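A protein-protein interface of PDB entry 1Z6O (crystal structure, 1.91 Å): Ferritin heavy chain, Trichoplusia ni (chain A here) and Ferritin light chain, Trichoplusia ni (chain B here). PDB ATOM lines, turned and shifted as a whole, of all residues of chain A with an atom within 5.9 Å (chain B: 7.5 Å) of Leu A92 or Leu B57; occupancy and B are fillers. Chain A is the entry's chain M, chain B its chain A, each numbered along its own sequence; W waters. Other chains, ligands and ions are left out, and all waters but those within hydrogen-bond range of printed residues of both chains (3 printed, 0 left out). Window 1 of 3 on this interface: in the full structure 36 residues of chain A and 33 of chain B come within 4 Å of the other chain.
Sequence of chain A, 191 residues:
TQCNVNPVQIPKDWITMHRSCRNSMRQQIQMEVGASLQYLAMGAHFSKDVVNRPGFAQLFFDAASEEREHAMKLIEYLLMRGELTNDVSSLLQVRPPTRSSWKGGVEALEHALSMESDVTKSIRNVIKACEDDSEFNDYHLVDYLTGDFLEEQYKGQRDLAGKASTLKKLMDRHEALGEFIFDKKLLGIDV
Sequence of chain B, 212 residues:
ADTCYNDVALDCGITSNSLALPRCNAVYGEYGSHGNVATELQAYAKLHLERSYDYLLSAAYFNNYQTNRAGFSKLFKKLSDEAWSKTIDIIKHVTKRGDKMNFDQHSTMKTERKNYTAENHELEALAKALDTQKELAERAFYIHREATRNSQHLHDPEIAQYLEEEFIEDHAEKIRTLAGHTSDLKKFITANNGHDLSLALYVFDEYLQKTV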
ATOM      1  N   ILE A  29       2.828 -19.950 -20.316  1.00  0.00           N
ATOM      2  CA  ILE A  29       2.474 -20.410 -18.973  1.00  0.00           C
ATOM      3  C   ILE A  29       2.882 -21.876 -18.802  1.00  0.00           C
ATOM      4  O   ILE A  29       3.476 -22.251 -17.783  1.00  0.00           O
ATOM      5  CB  ILE A  29       0.957 -20.200 -18.719  1.00  0.00           C
ATOM      6  CG1 ILE A  29       0.697 -18.698 -18.512  1.00  0.00           C
ATOM      7  CG2 ILE A  29       0.481 -21.007 -17.492  1.00  0.00           C
ATOM      8  CD1 ILE A  29      -0.788 -18.276 -18.659  1.00  0.00           C
ATOM      9  N   GLN A  30       2.597 -22.707 -19.803  1.00  0.00           N
ATOM     10  CA  GLN A  30       2.981 -24.118 -19.719  1.00  0.00           C
ATOM     11  C   GLN A  30       4.507 -24.240 -19.701  1.00  0.00           C
ATOM     12  O   GLN A  30       5.065 -25.088 -19.003  1.00  0.00           O
ATOM     13  CB  GLN A  30       2.411 -24.923 -20.907  1.00  0.00           C
ATOM     14  CG  GLN A  30       2.921 -26.385 -20.971  1.00  0.00           C
ATOM     15  CD  GLN A  30       2.543 -27.199 -19.732  1.00  0.00           C
ATOM     16  OE1 GLN A  30       1.386 -27.236 -19.341  1.00  0.00           O
ATOM     17  NE2 GLN A  30       3.524 -27.857 -19.118  1.00  0.00           N
ATOM     18  N   VAL A  33       5.820 -23.558 -16.203  1.00  0.00           N
ATOM     19  CA  VAL A  33       5.543 -24.703 -15.331  1.00  0.00           C
ATOM     20  C   VAL A  33       6.527 -25.832 -15.639  1.00  0.00           C
ATOM     21  O   VAL A  33       7.064 -26.461 -14.722  1.00  0.00           O
ATOM     22  CB  VAL A  33       4.069 -25.180 -15.491  1.00  0.00           C
ATOM     23  CG1 VAL A  33       3.857 -26.538 -14.793  1.00  0.00           C
ATOM     24  CG2 VAL A  33       3.135 -24.134 -14.866  1.00  0.00           C
ATOM     25  N   ALA A  71       4.833 -18.372 -13.745  1.00  0.00           N
ATOM     26  CA  ALA A  71       3.603 -18.891 -14.334  1.00  0.00           C
ATOM     27  C   ALA A  71       2.400 -18.162 -13.723  1.00  0.00           C
ATOM     28  O   ALA A  71       1.478 -17.752 -14.432  1.00  0.00           O
ATOM     29  CB  ALA A  71       3.483 -20.393 -14.074  1.00  0.00           C
ATOM     30  N   ILE A  75      -0.599 -15.835 -15.547  1.00  0.00           N
ATOM     31  CA  ILE A  75      -2.012 -16.162 -15.358  1.00  0.00           C
ATOM     32  C   ILE A  75      -2.747 -14.933 -14.797  1.00  0.00           C
ATOM     33  O   ILE A  75      -3.845 -14.594 -15.256  1.00  0.00           O
ATOM     34  CB  ILE A  75      -2.180 -17.359 -14.380  1.00  0.00           C
ATOM     35  CG1 ILE A  75      -1.695 -18.645 -15.066  1.00  0.00           C
ATOM     36  CG2 ILE A  75      -3.654 -17.487 -13.935  1.00  0.00           C
ATOM     37  CD1 ILE A  75      -1.526 -19.835 -14.105  1.00  0.00           C
ATOM     38  N   VAL A  88      -9.638 -22.952 -18.490  1.00  0.00           N
ATOM     39  CA  VAL A  88      -8.630 -22.863 -17.453  1.00  0.00           C
ATOM     40  C   VAL A  88      -7.994 -24.237 -17.217  1.00  0.00           C
ATOM     41  O   VAL A  88      -6.778 -24.346 -17.074  1.00  0.00           O
ATOM     42  CB  VAL A  88      -9.246 -22.336 -16.129  1.00  0.00           C
ATOM     43  CG1 VAL A  88      -8.192 -22.325 -15.035  1.00  0.00           C
ATOM     44  CG2 VAL A  88      -9.803 -20.911 -16.339  1.00  0.00           C
ATOM     45  N   SER A  89      -8.815 -25.283 -17.199  1.00  0.00           N
ATOM     46  CA  SER A  89      -8.316 -26.639 -16.943  1.00  0.00           C
ATOM     47  C   SER A  89      -7.230 -27.074 -17.921  1.00  0.00           C
ATOM     48  O   SER A  89      -6.288 -27.757 -17.544  1.00  0.00           O
ATOM     49  CB  SER A  89      -9.467 -27.650 -16.996  1.00  0.00           C
ATOM     50  OG  SER A  89     -10.423 -27.391 -15.982  1.00  0.00           O
ATOM     51  N   SER A  90      -7.356 -26.654 -19.173  1.00  0.00           N
ATOM     52  CA  SER A  90      -6.394 -27.023 -20.209  1.00  0.00           C
ATOM     53  C   SER A  90      -5.130 -26.164 -20.227  1.00  0.00           C
ATOM     54  O   SER A  90      -4.250 -26.384 -21.051  1.00  0.00           O
ATOM     55  CB  SER A  90      -7.068 -26.917 -21.578  1.00  0.00           C
ATOM     56  OG  SER A  90      -7.541 -25.591 -21.761  1.00  0.00           O
ATOM     57  N   LEU A  91      -5.028 -25.185 -19.333  1.00  0.00           N
ATOM     58  CA  LEU A  91      -3.850 -24.312 -19.327  1.00  0.00           C
ATOM     59  C   LEU A  91      -2.542 -25.014 -19.017  1.00  0.00           C
ATOM     60  O   LEU A  91      -1.500 -24.660 -19.560  1.00  0.00           O
ATOM     61  CB  LEU A  91      -3.998 -23.206 -18.281  1.00  0.00           C
ATOM     62  CG  LEU A  91      -4.338 -21.774 -18.622  1.00  0.00           C
ATOM     63  CD1 LEU A  91      -4.193 -20.962 -17.319  1.00  0.00           C
ATOM     64  CD2 LEU A  91      -3.417 -21.238 -19.733  1.00  0.00           C
ATOM     65  N   LEU A  92      -2.602 -26.003 -18.132  1.00  0.00           N
ATOM     66  CA  LEU A  92      -1.403 -26.695 -17.671  1.00  0.00           C
ATOM     67  C   LEU A  92      -1.501 -28.186 -17.613  1.00  0.00           C
ATOM     68  O   LEU A  92      -2.574 -28.746 -17.433  1.00  0.00           O
ATOM     69  CB  LEU A  92      -1.064 -26.259 -16.248  1.00  0.00           C
ATOM     70  CG  LEU A  92      -0.810 -24.795 -16.015  1.00  0.00           C
ATOM     71  CD1 LEU A  92      -0.724 -24.525 -14.524  1.00  0.00           C
ATOM     72  CD2 LEU A  92       0.472 -24.431 -16.738  1.00  0.00           C
ATOM     73  N   GLN A  93      -0.342 -28.818 -17.715  1.00  0.00           N
ATOM     74  CA  GLN A  93      -0.240 -30.262 -17.620  1.00  0.00           C
ATOM     75  C   GLN A  93       1.079 -30.536 -16.889  1.00  0.00           C
ATOM     76  O   GLN A  93       2.128 -30.028 -17.276  1.00  0.00           O
ATOM     77  CB  GLN A  93      -0.225 -30.884 -19.017  1.00  0.00           C
ATOM     78  CG  GLN A  93      -0.224 -32.409 -19.023  1.00  0.00           C
ATOM     79  CD  GLN A  93      -1.391 -33.014 -18.249  1.00  0.00           C
ATOM     80  OE1 GLN A  93      -2.560 -32.761 -18.560  1.00  0.00           O
ATOM     81  NE2 GLN A  93      -1.077 -33.821 -17.236  1.00  0.00           N
ATOM     82  N   VAL A  94       1.015 -31.292 -15.801  1.00  0.00           N
ATOM     83  CA  VAL A  94       2.216 -31.642 -15.057  1.00  0.00           C
ATOM     84  C   VAL A  94       2.697 -32.986 -15.608  1.00  0.00           C
ATOM     85  O   VAL A  94       1.934 -33.945 -15.652  1.00  0.00           O
ATOM     86  CB  VAL A  94       1.911 -31.793 -13.546  1.00  0.00           C
ATOM     87  CG1 VAL A  94       3.095 -32.429 -12.826  1.00  0.00           C
ATOM     88  CG2 VAL A  94       1.599 -30.434 -12.947  1.00  0.00           C
ATOM     89  N   GLU B  50       1.073 -32.595  -8.463  1.00  0.00           N
ATOM     90  CA  GLU B  50      -0.061 -32.496  -9.376  1.00  0.00           C
ATOM     91  C   GLU B  50      -1.194 -31.706  -8.737  1.00  0.00           C
ATOM     92  O   GLU B  50      -1.785 -30.832  -9.373  1.00  0.00           O
ATOM     93  CB  GLU B  50      -0.562 -33.901  -9.759  1.00  0.00           C
ATOM     94  CG  GLU B  50       0.509 -34.706 -10.498  1.00  0.00           C
ATOM     95  CD  GLU B  50       0.172 -36.189 -10.657  1.00  0.00           C
ATOM     96  OE1 GLU B  50      -0.625 -36.724  -9.847  1.00  0.00           O
ATOM     97  OE2 GLU B  50       0.733 -36.821 -11.582  1.00  0.00           O
ATOM     98  N   ARG B  51      -1.512 -32.009  -7.484  1.00  0.00           N
ATOM     99  CA  ARG B  51      -2.592 -31.278  -6.833  1.00  0.00           C
ATOM    100  C   ARG B  51      -2.249 -29.805  -6.626  1.00  0.00           C
ATOM    101  O   ARG B  51      -3.150 -28.966  -6.686  1.00  0.00           O
ATOM    102  CB  ARG B  51      -2.965 -31.908  -5.482  1.00  0.00           C
ATOM    103  CG  ARG B  51      -3.646 -33.263  -5.596  1.00  0.00           C
ATOM    104  CD  ARG B  51      -4.907 -33.206  -6.465  1.00  0.00           C
ATOM    105  NE  ARG B  51      -5.558 -34.515  -6.503  1.00  0.00           N
ATOM    106  CZ  ARG B  51      -6.266 -34.975  -7.528  1.00  0.00           C
ATOM    107  NH1 ARG B  51      -6.424 -34.233  -8.619  1.00  0.00           N
ATOM    108  NH2 ARG B  51      -6.806 -36.188  -7.467  1.00  0.00           N
ATOM    109  N   SER B  52      -0.973 -29.474  -6.388  1.00  0.00           N
ATOM    110  CA  SER B  52      -0.644 -28.062  -6.191  1.00  0.00           C
ATOM    111  C   SER B  52      -1.050 -27.267  -7.427  1.00  0.00           C
ATOM    112  O   SER B  52      -1.609 -26.175  -7.309  1.00  0.00           O
ATOM    113  CB  SER B  52       0.853 -27.832  -5.881  1.00  0.00           C
ATOM    114  OG  SER B  52       1.689 -28.059  -7.003  1.00  0.00           O
ATOM    115  N   TYR B  53      -0.781 -27.808  -8.610  1.00  0.00           N
ATOM    116  CA  TYR B  53      -1.157 -27.106  -9.834  1.00  0.00           C
ATOM    117  C   TYR B  53      -2.669 -27.165 -10.106  1.00  0.00           C
ATOM    118  O   TYR B  53      -3.223 -26.220 -10.662  1.00  0.00           O
ATOM    119  CB  TYR B  53      -0.311 -27.612 -11.024  1.00  0.00           C
ATOM    120  CG  TYR B  53       1.033 -26.898 -11.070  1.00  0.00           C
ATOM    121  CD1 TYR B  53       2.232 -27.561 -10.764  1.00  0.00           C
ATOM    122  CD2 TYR B  53       1.094 -25.540 -11.382  1.00  0.00           C
ATOM    123  CE1 TYR B  53       3.460 -26.874 -10.774  1.00  0.00           C
ATOM    124  CE2 TYR B  53       2.305 -24.851 -11.390  1.00  0.00           C
ATOM    125  CZ  TYR B  53       3.478 -25.517 -11.091  1.00  0.00           C
ATOM    126  OH  TYR B  53       4.658 -24.813 -11.136  1.00  0.00           O
ATOM    127  N   ASP B  54      -3.352 -28.239  -9.702  1.00  0.00           N
ATOM    128  CA  ASP B  54      -4.817 -28.286  -9.867  1.00  0.00           C
ATOM    129  C   ASP B  54      -5.433 -27.159  -9.012  1.00  0.00           C
ATOM    130  O   ASP B  54      -6.315 -26.425  -9.456  1.00  0.00           O
ATOM    131  CB  ASP B  54      -5.421 -29.611  -9.357  1.00  0.00           C
ATOM    132  CG  ASP B  54      -5.108 -30.798 -10.253  1.00  0.00           C
ATOM    133  OD1 ASP B  54      -4.892 -30.590 -11.462  1.00  0.00           O
ATOM    134  OD2 ASP B  54      -5.097 -31.944  -9.745  1.00  0.00           O
ATOM    135  N   TYR B  55      -4.981 -27.046  -7.767  1.00  0.00           N
ATOM    136  CA  TYR B  55      -5.501 -26.013  -6.867  1.00  0.00           C
ATOM    137  C   TYR B  55      -5.171 -24.615  -7.399  1.00  0.00           C
ATOM    138  O   TYR B  55      -5.956 -23.676  -7.245  1.00  0.00           O
ATOM    139  CB  TYR B  55      -4.901 -26.183  -5.464  1.00  0.00           C
ATOM    140  CG  TYR B  55      -5.338 -27.462  -4.763  1.00  0.00           C
ATOM    141  CD1 TYR B  55      -4.480 -28.116  -3.888  1.00  0.00           C
ATOM    142  CD2 TYR B  55      -6.621 -27.992  -4.955  1.00  0.00           C
ATOM    143  CE1 TYR B  55      -4.879 -29.274  -3.206  1.00  0.00           C
ATOM    144  CE2 TYR B  55      -7.035 -29.154  -4.275  1.00  0.00           C
ATOM    145  CZ  TYR B  55      -6.151 -29.781  -3.401  1.00  0.00           C
ATOM    146  OH  TYR B  55      -6.530 -30.912  -2.703  1.00  0.00           O
ATOM    147  N   LEU B  56      -3.998 -24.472  -8.003  1.00  0.00           N
ATOM    148  CA  LEU B  56      -3.610 -23.178  -8.553  1.00  0.00           C
ATOM    149  C   LEU B  56      -4.591 -22.769  -9.657  1.00  0.00           C
ATOM    150  O   LEU B  56      -4.980 -21.602  -9.749  1.00  0.00           O
ATOM    151  CB  LEU B  56      -2.177 -23.247  -9.107  1.00  0.00           C
ATOM    152  CG  LEU B  56      -1.676 -21.920  -9.695  1.00  0.00           C
ATOM    153  CD1 LEU B  56      -1.623 -20.883  -8.580  1.00  0.00           C
ATOM    154  CD2 LEU B  56      -0.288 -22.096 -10.298  1.00  0.00           C
ATOM    155  N   LEU B  57      -4.999 -23.721 -10.494  1.00  0.00           N
ATOM    156  CA  LEU B  57      -5.949 -23.414 -11.566  1.00  0.00           C
ATOM    157  C   LEU B  57      -7.320 -23.053 -10.987  1.00  0.00           C
ATOM    158  O   LEU B  57      -8.010 -22.195 -11.530  1.00  0.00           O
ATOM    159  CB  LEU B  57      -6.068 -24.592 -12.547  1.00  0.00           C
ATOM    160  CG  LEU B  57      -4.774 -24.874 -13.341  1.00  0.00           C
ATOM    161  CD1 LEU B  57      -4.967 -26.122 -14.199  1.00  0.00           C
ATOM    162  CD2 LEU B  57      -4.415 -23.674 -14.216  1.00  0.00           C
ATOM    163  N   SER B  58      -7.730 -23.707  -9.902  1.00  0.00           N
ATOM    164  CA  SER B  58      -9.004 -23.345  -9.271  1.00  0.00           C
ATOM    165  C   SER B  58      -8.891 -21.931  -8.698  1.00  0.00           C
ATOM    166  O   SER B  58      -9.835 -21.146  -8.792  1.00  0.00           O
ATOM    167  CB  SER B  58      -9.365 -24.314  -8.133  1.00  0.00           C
ATOM    168  OG  SER B  58      -9.781 -25.564  -8.652  1.00  0.00           O
ATOM    169  N   ALA B  59      -7.748 -21.602  -8.094  1.00  0.00           N
ATOM    170  CA  ALA B  59      -7.568 -20.259  -7.541  1.00  0.00           C
ATOM    171  C   ALA B  59      -7.691 -19.224  -8.666  1.00  0.00           C
ATOM    172  O   ALA B  59      -8.293 -18.160  -8.483  1.00  0.00           O
ATOM    173  CB  ALA B  59      -6.200 -20.131  -6.863  1.00  0.00           C
ATOM    174  N   ALA B  60      -7.118 -19.539  -9.825  1.00  0.00           N
ATOM    175  CA  ALA B  60      -7.182 -18.635 -10.977  1.00  0.00           C
ATOM    176  C   ALA B  60      -8.627 -18.491 -11.449  1.00  0.00           C
ATOM    177  O   ALA B  60      -9.113 -17.381 -11.662  1.00  0.00           O
ATOM    178  CB  ALA B  60      -6.304 -19.176 -12.135  1.00  0.00           C
ATOM    179  N   TYR B  61      -9.323 -19.614 -11.604  1.00  0.00           N
ATOM    180  CA  TYR B  61     -10.706 -19.560 -12.062  1.00  0.00           C
ATOM    181  C   TYR B  61     -11.580 -18.667 -11.173  1.00  0.00           C
ATOM    182  O   TYR B  61     -12.376 -17.875 -11.677  1.00  0.00           O
ATOM    183  CB  TYR B  61     -11.318 -20.960 -12.117  1.00  0.00           C
ATOM    184  CG  TYR B  61     -12.739 -20.953 -12.632  1.00  0.00           C
ATOM    185  CD1 TYR B  61     -13.009 -20.695 -13.977  1.00  0.00           C
ATOM    186  CD2 TYR B  61     -13.819 -21.174 -11.771  1.00  0.00           C
ATOM    187  CE1 TYR B  61     -14.320 -20.656 -14.457  1.00  0.00           C
ATOM    188  CE2 TYR B  61     -15.138 -21.136 -12.242  1.00  0.00           C
ATOM    189  CZ  TYR B  61     -15.373 -20.878 -13.585  1.00  0.00           C
ATOM    190  OH  TYR B  61     -16.656 -20.842 -14.061  1.00  0.00           O
ATOM    191  N   PHE B  62     -11.443 -18.793  -9.857  1.00  0.00           N
ATOM    192  CA  PHE B  62     -12.251 -17.969  -8.966  1.00  0.00           C
ATOM    193  C   PHE B  62     -11.818 -16.518  -8.899  1.00  0.00           C
ATOM    194  O   PHE B  62     -12.462 -15.699  -8.244  1.00  0.00           O
ATOM    195  CB  PHE B  62     -12.316 -18.595  -7.566  1.00  0.00           C
ATOM    196  CG  PHE B  62     -13.288 -19.740  -7.501  1.00  0.00           C
ATOM    197  CD1 PHE B  62     -12.844 -21.057  -7.524  1.00  0.00           C
ATOM    198  CD2 PHE B  62     -14.659 -19.491  -7.542  1.00  0.00           C
ATOM    199  CE1 PHE B  62     -13.758 -22.120  -7.598  1.00  0.00           C
ATOM    200  CE2 PHE B  62     -15.579 -20.538  -7.618  1.00  0.00           C
ATOM    201  CZ  PHE B  62     -15.126 -21.855  -7.648  1.00  0.00           C
ATOM    202  N   ASN B  63     -10.727 -16.197  -9.587  1.00  0.00           N
ATOM    203  CA  ASN B  63     -10.261 -14.819  -9.629  1.00  0.00           C
ATOM    204  C   ASN B  63     -10.537 -14.194 -11.011  1.00  0.00           C
ATOM    205  O   ASN B  63      -9.996 -13.129 -11.322  1.00  0.00           O
ATOM    206  CB  ASN B  63      -8.761 -14.743  -9.275  1.00  0.00           C
ATOM    207  CG  ASN B  63      -8.283 -13.313  -9.002  1.00  0.00           C
ATOM    208  OD1 ASN B  63      -8.991 -12.509  -8.392  1.00  0.00           O
ATOM    209  ND2 ASN B  63      -7.066 -13.001  -9.442  1.00  0.00           N
ATOM    210  N   PHE B  76      -8.139 -21.732  -2.336  1.00  0.00           N
ATOM    211  CA  PHE B  76      -7.398 -22.601  -3.245  1.00  0.00           C
ATOM    212  C   PHE B  76      -5.931 -22.240  -3.376  1.00  0.00           C
ATOM    213  O   PHE B  76      -5.089 -23.114  -3.555  1.00  0.00           O
ATOM    214  CB  PHE B  76      -8.057 -22.625  -4.623  1.00  0.00           C
ATOM    215  CG  PHE B  76      -9.246 -23.531  -4.683  1.00  0.00           C
ATOM    216  CD1 PHE B  76     -10.540 -23.014  -4.683  1.00  0.00           C
ATOM    217  CD2 PHE B  76      -9.069 -24.916  -4.691  1.00  0.00           C
ATOM    218  CE1 PHE B  76     -11.652 -23.871  -4.686  1.00  0.00           C
ATOM    219  CE2 PHE B  76     -10.168 -25.782  -4.697  1.00  0.00           C
ATOM    220  CZ  PHE B  76     -11.463 -25.254  -4.694  1.00  0.00           C
ATOM    221  N   SER B  80      -2.869 -24.725  -2.726  1.00  0.00           N
ATOM    222  CA  SER B  80      -1.816 -24.876  -3.737  1.00  0.00           C
ATOM    223  C   SER B  80      -0.431 -24.648  -3.135  1.00  0.00           C
ATOM    224  O   SER B  80       0.487 -25.454  -3.341  1.00  0.00           O
ATOM    225  CB  SER B  80      -2.025 -23.876  -4.888  1.00  0.00           C
ATOM    226  OG  SER B  80      -0.965 -23.988  -5.834  1.00  0.00           O
ATOM    227  N   TYR B 116      -9.310 -33.508 -12.944  1.00  0.00           N
ATOM    228  CA  TYR B 116      -9.642 -32.369 -12.098  1.00  0.00           C
ATOM    229  C   TYR B 116     -10.023 -31.216 -13.021  1.00  0.00           C
ATOM    230  O   TYR B 116      -9.228 -30.817 -13.862  1.00  0.00           O
ATOM    231  CB  TYR B 116      -8.419 -31.970 -11.259  1.00  0.00           C
ATOM    232  CG  TYR B 116      -8.673 -30.855 -10.262  1.00  0.00           C
ATOM    233  CD1 TYR B 116      -8.840 -31.137  -8.906  1.00  0.00           C
ATOM    234  CD2 TYR B 116      -8.721 -29.516 -10.674  1.00  0.00           C
ATOM    235  CE1 TYR B 116      -9.042 -30.113  -7.966  1.00  0.00           C
ATOM    236  CE2 TYR B 116      -8.926 -28.477  -9.745  1.00  0.00           C
ATOM    237  CZ  TYR B 116      -9.080 -28.789  -8.393  1.00  0.00           C
ATOM    238  OH  TYR B 116      -9.243 -27.784  -7.461  1.00  0.00           O
ATOM    239  N   THR B 117     -11.233 -30.688 -12.890  1.00  0.00           N
ATOM    240  CA  THR B 117     -11.636 -29.558 -13.728  1.00  0.00           C
ATOM    241  C   THR B 117     -11.714 -28.336 -12.823  1.00  0.00           C
ATOM    242  O   THR B 117     -12.285 -28.396 -11.736  1.00  0.00           O
ATOM    243  CB  THR B 117     -13.008 -29.781 -14.396  1.00  0.00           C
ATOM    244  OG1 THR B 117     -14.042 -29.686 -13.417  1.00  0.00           O
ATOM    245  CG2 THR B 117     -13.068 -31.151 -15.043  1.00  0.00           C
ATOM    246  N   ALA B 118     -11.138 -27.228 -13.272  1.00  0.00           N
ATOM    247  CA  ALA B 118     -11.116 -26.004 -12.478  1.00  0.00           C
ATOM    248  C   ALA B 118     -12.372 -25.146 -12.602  1.00  0.00           C
ATOM    249  O   ALA B 118     -12.686 -24.381 -11.689  1.00  0.00           O
ATOM    250  CB  ALA B 118      -9.882 -25.175 -12.849  1.00  0.00           C
ATOM    251  N   GLU B 119     -13.091 -25.265 -13.719  1.00  0.00           N
ATOM    252  CA  GLU B 119     -14.304 -24.459 -13.916  1.00  0.00           C
ATOM    253  C   GLU B 119     -15.489 -25.106 -13.202  1.00  0.00           C
ATOM    254  O   GLU B 119     -16.123 -26.007 -13.741  1.00  0.00           O
ATOM    255  CB  GLU B 119     -14.623 -24.317 -15.416  1.00  0.00           C
ATOM    256  CG  GLU B 119     -13.464 -23.790 -16.262  1.00  0.00           C
ATOM    257  CD  GLU B 119     -12.510 -24.883 -16.749  1.00  0.00           C
ATOM    258  OE1 GLU B 119     -12.637 -26.050 -16.317  1.00  0.00           O
ATOM    259  OE2 GLU B 119     -11.619 -24.572 -17.570  1.00  0.00           O
HETATM  260  O   HOH W   1      -0.015 -35.476 -14.243  1.00  0.00           O
HETATM  261  O   HOH W   2      -6.364 -29.537 -15.207  1.00  0.00           O
HETATM  262  O   HOH W   3       2.949 -36.178 -13.259  1.00  0.00           O
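Of the 20 printed residues of chain B, 7 touch a printed residue of chain A.
Printed residues of chain B that touch a printed residue of chain A: Tyr B53, Leu B57, Ala B60, Tyr B61, Thr B117, Ala B118 and Glu B119.
Hydrophobic or aromatic side chains of chain B within 4 Å of the printed part of chain A: Tyr B53, Leu B57, Ala B60, Tyr B61 and Ala B118.
Along chain B the printed residues that touch a printed residue of chain A span positions 53 to 119.
Of the 12 printed residues of chain A, 6 touch a printed residue of chain B.
Hydrophobic or aromatic side chains of chain A that line the printed part of chain B: Val A33, Ile A75, Val A88, Leu A92 and Val A94.
Among the printed residues, 13 pairs touch across the chains.
Among the printed residues, no Asp or Glu carboxylate lies within 4 Å of a Lys or Arg side-chain nitrogen of the other chain.
OG of Ser A89 is in hydrogen-bond range of N of Ala B118 (2.8 Å).
The side-chain carboxylate (OE1) of Glu B119 lies within hydrogen-bond range of the side-chain hydroxyl (OG) of Ser A89 (2.6 Å).
The backbone NH (N) of Val A88 is in hydrogen-bond range of the side-chain carboxylate (OE2) of Glu B119, 2.7 Å away.
Tyr B53 touches Val A33 (CE2 to CG2, 3.6 Å).
CG2 of Ile A75 touches CB of Ala B60, at 3.6 Å.
Val A88 touches Leu B57.
Val A88 touches Tyr B61.
Val A88 touches Ala B118.
Ser A89 touches Leu B57 (O to CD1, 3.95 Å).
Ser A89 touches Thr B117.
Leu A92 touches Tyr B53.
Leu B57 touches Leu A92 (CD2 to CD1, 3.8 Å).
Val A94 touches Tyr B53 (CG2 to CD1, 3.7 Å).
Water W1 lies within hydrogen-bond range of O of Val A94 (2.9 Å) and OE2 of Glu B50 (3.1 Å).
Water W3 bridges the side-chain carboxylate (OE2) of Glu B50 (2.9 Å) and the backbone carbonyl oxygen (O) of Val A94 (3.4 Å).
Water W2 bridges the backbone carbonyl oxygen of Ser A89 and the backbone carbonyl oxygen of Tyr B116.
Of chain B, only Tyr B53 and Leu B57 come within 4 Å of Leu A92.
Leu B57 touches just these residues of chain A: Val A88, Ser A89 and Leu A92.
Of the printed residues of chain A, Tyr B61 touches Val A88.
Printed residues of chain B within 4 Å of Val A33: Tyr B53 (3.6 Å).
Of the printed residues of chain B, Ser A89 touches Leu B57, Thr B117, Ala B118 and Glu B119.
Printed residues of chain A within 4 Å of Glu B119: Val A88 and Ser A89.
The nearest residue of chain A that does not touch Leu B57 is Leu A91 (4.1 Å).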
